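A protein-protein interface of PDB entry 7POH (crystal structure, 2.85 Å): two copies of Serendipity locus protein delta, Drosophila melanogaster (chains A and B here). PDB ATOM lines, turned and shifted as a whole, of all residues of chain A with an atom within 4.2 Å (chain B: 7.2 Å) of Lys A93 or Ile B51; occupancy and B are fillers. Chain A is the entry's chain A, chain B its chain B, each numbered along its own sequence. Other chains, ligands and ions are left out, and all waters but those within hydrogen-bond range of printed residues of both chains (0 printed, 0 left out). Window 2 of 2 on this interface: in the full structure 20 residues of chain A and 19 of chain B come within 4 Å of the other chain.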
ATOM      1  N   THR A  89      18.744  14.474  -7.246  1.00  0.00           N
ATOM      2  CA  THR A  89      17.379  13.898  -7.256  1.00  0.00           C
ATOM      3  C   THR A  89      16.493  14.807  -6.411  1.00  0.00           C
ATOM      4  O   THR A  89      15.421  15.090  -6.904  1.00  0.00           O
ATOM      5  CB  THR A  89      17.288  12.470  -6.726  1.00  0.00           C
ATOM      6  OG1 THR A  89      17.731  12.578  -5.378  1.00  0.00           O
ATOM      7  CG2 THR A  89      18.103  11.478  -7.522  1.00  0.00           C
ATOM      8  N   THR A  90      16.932  15.305  -5.242  1.00  0.00           N
ATOM      9  CA  THR A  90      16.025  16.109  -4.363  1.00  0.00           C
ATOM     10  C   THR A  90      15.670  17.444  -5.029  1.00  0.00           C
ATOM     11  O   THR A  90      14.540  17.929  -4.824  1.00  0.00           O
ATOM     12  CB  THR A  90      16.539  16.342  -2.939  1.00  0.00           C
ATOM     13  OG1 THR A  90      17.572  17.286  -3.099  1.00  0.00           O
ATOM     14  CG2 THR A  90      16.999  15.085  -2.224  1.00  0.00           C
ATOM     15  N   GLN A  91      16.602  17.974  -5.807  1.00  0.00           N
ATOM     16  CA  GLN A  91      16.400  19.115  -6.732  1.00  0.00           C
ATOM     17  C   GLN A  91      15.325  18.781  -7.770  1.00  0.00           C
ATOM     18  O   GLN A  91      14.455  19.609  -8.029  1.00  0.00           O
ATOM     19  CB  GLN A  91      17.724  19.456  -7.433  1.00  0.00           C
ATOM     20  CG  GLN A  91      17.624  20.574  -8.463  1.00  0.00           C
ATOM     21  CD  GLN A  91      17.118  21.838  -7.823  1.00  0.00           C
ATOM     22  OE1 GLN A  91      17.236  21.997  -6.600  1.00  0.00           O
ATOM     23  NE2 GLN A  91      16.523  22.718  -8.629  1.00  0.00           N
ATOM     24  N   LEU A  92      15.413  17.624  -8.392  1.00  0.00           N
ATOM     25  CA  LEU A  92      14.398  17.192  -9.386  1.00  0.00           C
ATOM     26  C   LEU A  92      12.987  17.228  -8.768  1.00  0.00           C
ATOM     27  O   LEU A  92      12.138  17.787  -9.419  1.00  0.00           O
ATOM     28  CB  LEU A  92      14.785  15.802  -9.898  1.00  0.00           C
ATOM     29  CG  LEU A  92      14.216  15.378 -11.238  1.00  0.00           C
ATOM     30  CD1 LEU A  92      14.313  16.476 -12.268  1.00  0.00           C
ATOM     31  CD2 LEU A  92      14.953  14.160 -11.736  1.00  0.00           C
ATOM     32  N   LYS A  93      12.802  16.797  -7.513  1.00  0.00           N
ATOM     33  CA  LYS A  93      11.500  16.729  -6.777  1.00  0.00           C
ATOM     34  C   LYS A  93      10.898  18.129  -6.557  1.00  0.00           C
ATOM     35  O   LYS A  93       9.667  18.230  -6.630  1.00  0.00           O
ATOM     36  CB  LYS A  93      11.655  15.999  -5.429  1.00  0.00           C
ATOM     37  CG  LYS A  93      12.191  14.556  -5.510  1.00  0.00           C
ATOM     38  CD  LYS A  93      11.904  13.572  -4.350  1.00  0.00           C
ATOM     39  CE  LYS A  93      11.795  14.170  -2.955  1.00  0.00           C
ATOM     40  NZ  LYS A  93      13.036  14.849  -2.496  1.00  0.00           N
ATOM     41  N   LEU A  94      11.735  19.152  -6.337  1.00  0.00           N
ATOM     42  CA  LEU A  94      11.399  20.593  -6.048  1.00  0.00           C
ATOM     43  C   LEU A  94      10.467  21.277  -7.075  1.00  0.00           C
ATOM     44  O   LEU A  94      10.253  20.705  -8.152  1.00  0.00           O
ATOM     45  CB  LEU A  94      12.715  21.384  -5.931  1.00  0.00           C
ATOM     46  CG  LEU A  94      13.210  21.738  -4.527  1.00  0.00           C
ATOM     47  CD1 LEU A  94      12.956  20.656  -3.487  1.00  0.00           C
ATOM     48  CD2 LEU A  94      14.687  22.051  -4.558  1.00  0.00           C
ATOM     49  N   PHE B   9      15.508  22.559 -14.874  1.00  0.00           N
ATOM     50  CA  PHE B   9      15.956  21.812 -13.684  1.00  0.00           C
ATOM     51  C   PHE B   9      16.022  22.701 -12.440  1.00  0.00           C
ATOM     52  O   PHE B   9      15.987  22.167 -11.326  1.00  0.00           O
ATOM     53  CB  PHE B   9      17.322  21.231 -14.040  1.00  0.00           C
ATOM     54  CG  PHE B   9      17.848  20.234 -13.045  1.00  0.00           C
ATOM     55  CD1 PHE B   9      17.278  18.970 -12.948  1.00  0.00           C
ATOM     56  CD2 PHE B   9      18.910  20.551 -12.222  1.00  0.00           C
ATOM     57  CE1 PHE B   9      17.740  18.065 -12.010  1.00  0.00           C
ATOM     58  CE2 PHE B   9      19.407  19.619 -11.333  1.00  0.00           C
ATOM     59  CZ  PHE B   9      18.810  18.396 -11.207  1.00  0.00           C
ATOM     60  N   HIS B  46      18.068   9.004 -16.195  1.00  0.00           N
ATOM     61  CA  HIS B  46      18.761   8.248 -15.119  1.00  0.00           C
ATOM     62  C   HIS B  46      18.331   8.761 -13.734  1.00  0.00           C
ATOM     63  O   HIS B  46      17.886   7.938 -12.890  1.00  0.00           O
ATOM     64  CB  HIS B  46      20.280   8.218 -15.338  1.00  0.00           C
ATOM     65  CG  HIS B  46      21.030   7.747 -14.137  1.00  0.00           C
ATOM     66  ND1 HIS B  46      20.568   6.732 -13.314  1.00  0.00           N
ATOM     67  CD2 HIS B  46      22.188   8.161 -13.602  1.00  0.00           C
ATOM     68  CE1 HIS B  46      21.406   6.554 -12.324  1.00  0.00           C
ATOM     69  NE2 HIS B  46      22.398   7.424 -12.472  1.00  0.00           N
ATOM     70  N   LEU B  47      18.421  10.065 -13.491  1.00  0.00           N
ATOM     71  CA  LEU B  47      18.109  10.626 -12.145  1.00  0.00           C
ATOM     72  C   LEU B  47      16.629  10.409 -11.800  1.00  0.00           C
ATOM     73  O   LEU B  47      16.330  10.195 -10.605  1.00  0.00           O
ATOM     74  CB  LEU B  47      18.500  12.105 -12.082  1.00  0.00           C
ATOM     75  CG  LEU B  47      20.006  12.368 -12.040  1.00  0.00           C
ATOM     76  CD1 LEU B  47      20.316  13.837 -12.302  1.00  0.00           C
ATOM     77  CD2 LEU B  47      20.600  11.916 -10.709  1.00  0.00           C
ATOM     78  N   ALA B  48      15.732  10.437 -12.786  1.00  0.00           N
ATOM     79  CA  ALA B  48      14.300  10.207 -12.524  1.00  0.00           C
ATOM     80  C   ALA B  48      14.149   8.766 -12.033  1.00  0.00           C
ATOM     81  O   ALA B  48      13.483   8.573 -10.960  1.00  0.00           O
ATOM     82  CB  ALA B  48      13.476  10.493 -13.751  1.00  0.00           C
ATOM     83  N   ASN B  49      14.793   7.811 -12.732  1.00  0.00           N
ATOM     84  CA  ASN B  49      14.770   6.379 -12.327  1.00  0.00           C
ATOM     85  C   ASN B  49      15.101   6.301 -10.848  1.00  0.00           C
ATOM     86  O   ASN B  49      14.289   5.744 -10.120  1.00  0.00           O
ATOM     87  CB  ASN B  49      15.783   5.449 -13.000  1.00  0.00           C
ATOM     88  CG  ASN B  49      15.527   5.232 -14.470  1.00  0.00           C
ATOM     89  OD1 ASN B  49      14.381   5.224 -14.912  1.00  0.00           O
ATOM     90  ND2 ASN B  49      16.598   5.051 -15.224  1.00  0.00           N
ATOM     91  N   CYS B  50      16.200   6.921 -10.421  1.00  0.00           N
ATOM     92  CA  CYS B  50      16.688   6.786  -9.028  1.00  0.00           C
ATOM     93  C   CYS B  50      15.566   7.049  -8.008  1.00  0.00           C
ATOM     94  O   CYS B  50      15.617   6.406  -6.963  1.00  0.00           O
ATOM     95  CB  CYS B  50      17.914   7.647  -8.763  1.00  0.00           C
ATOM     96  SG  CYS B  50      19.396   7.049  -9.607  1.00  0.00           S
ATOM     97  N   ILE B  51      14.558   7.884  -8.295  1.00  0.00           N
ATOM     98  CA  ILE B  51      13.425   8.153  -7.349  1.00  0.00           C
ATOM     99  C   ILE B  51      12.104   7.627  -7.934  1.00  0.00           C
ATOM    100  O   ILE B  51      11.037   8.204  -7.610  1.00  0.00           O
ATOM    101  CB  ILE B  51      13.410   9.645  -6.978  1.00  0.00           C
ATOM    102  CG1 ILE B  51      13.293  10.555  -8.209  1.00  0.00           C
ATOM    103  CG2 ILE B  51      14.642   9.972  -6.154  1.00  0.00           C
ATOM    104  CD1 ILE B  51      12.611  11.879  -7.928  1.00  0.00           C
ATOM    105  N   GLN B  52      12.188   6.491  -8.647  1.00  0.00           N
ATOM    106  CA  GLN B  52      11.126   5.794  -9.429  1.00  0.00           C
ATOM    107  C   GLN B  52      10.071   6.829  -9.833  1.00  0.00           C
ATOM    108  O   GLN B  52       8.931   6.758  -9.360  1.00  0.00           O
ATOM    109  CB  GLN B  52      10.609   4.531  -8.709  1.00  0.00           C
ATOM    110  CG  GLN B  52      10.566   4.600  -7.181  1.00  0.00           C
ATOM    111  CD  GLN B  52      11.831   4.170  -6.458  1.00  0.00           C
ATOM    112  OE1 GLN B  52      12.729   3.537  -7.013  1.00  0.00           O
ATOM    113  NE2 GLN B  52      11.922   4.507  -5.179  1.00  0.00           N
ATOM    114  N   THR B  53      10.508   7.832 -10.597  1.00  0.00           N
ATOM    115  CA  THR B  53       9.646   8.735 -11.403  1.00  0.00           C
ATOM    116  C   THR B  53      10.194   8.748 -12.841  1.00  0.00           C
ATOM    117  O   THR B  53      11.202   8.044 -13.129  1.00  0.00           O
ATOM    118  CB  THR B  53       9.521  10.147 -10.799  1.00  0.00           C
ATOM    119  OG1 THR B  53      10.645  10.922 -11.211  1.00  0.00           O
ATOM    120  CG2 THR B  53       9.429  10.192  -9.288  1.00  0.00           C
ATOM    121  N   GLN B  54       9.515   9.483 -13.715  1.00  0.00           N
ATOM    122  CA  GLN B  54       9.903   9.694 -15.133  1.00  0.00           C
ATOM    123  C   GLN B  54       9.378  11.080 -15.512  1.00  0.00           C
ATOM    124  O   GLN B  54       8.586  11.642 -14.729  1.00  0.00           O
ATOM    125  CB  GLN B  54       9.426   8.540 -16.034  1.00  0.00           C
ATOM    126  CG  GLN B  54       7.934   8.499 -16.362  1.00  0.00           C
ATOM    127  CD  GLN B  54       7.034   8.371 -15.153  1.00  0.00           C
ATOM    128  OE1 GLN B  54       6.808   9.329 -14.404  1.00  0.00           O
ATOM    129  NE2 GLN B  54       6.504   7.173 -14.953  1.00  0.00           N
ATOM    130  N   LEU B  55       9.832  11.609 -16.646  1.00  0.00           N
ATOM    131  CA  LEU B  55       9.737  13.048 -17.000  1.00  0.00           C
ATOM    132  C   LEU B  55       9.144  13.168 -18.403  1.00  0.00           C
ATOM    133  O   LEU B  55       9.475  12.354 -19.260  1.00  0.00           O
ATOM    134  CB  LEU B  55      11.137  13.682 -16.966  1.00  0.00           C
ATOM    135  CG  LEU B  55      12.050  13.359 -15.772  1.00  0.00           C
ATOM    136  CD1 LEU B  55      13.513  13.542 -16.167  1.00  0.00           C
ATOM    137  CD2 LEU B  55      11.683  14.193 -14.540  1.00  0.00           C
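Lys A93 touches one residue of chain B.
Printed residues of chain B within 4 Å of Thr A89: Leu B47 and Ile B51.
Printed residues of chain A within 4 Å of Ala B48: Leu A92 (3.9 Å).
Printed residues of chain A within 4 Å of Phe B9: Gln A91 and Leu A92.
Thr B53 touches none of the printed residues of chain A.
Thr A90 touches none of the printed residues of chain B.
The nearest residue of chain B that does not touch Lys A93 is Thr B53 (6.4 Å).
Among the printed residues, pairs that only touch across the chains: Lys A93 with Ile B51 (3.6 Å), Thr A89 with Ile B51 (3.7 Å), Thr A89 with Leu B47 (3.8 Å), Leu A92 with Phe B9 (3.8 Å) and Leu A92 with Ala B48 (3.9 Å).
No position is printed for both chains.
The backbone carbonyl oxygen of Phe B9 sits at hydrogen-bond distance from the side-chain amide nitrogen of Gln A91.
O of Ala B48 is in hydrogen-bond range of N of Thr B53 (3.1 Å).
Hydrophobic or aromatic side chains of chain A within 4 Å of the printed part of chain B: Leu A92.
Among the printed residues, 6 pairs touch across the chains.
Among the printed residues, no Asp or Glu carboxylate lies within 4 Å of a Lys or Arg side-chain nitrogen of the other chain.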
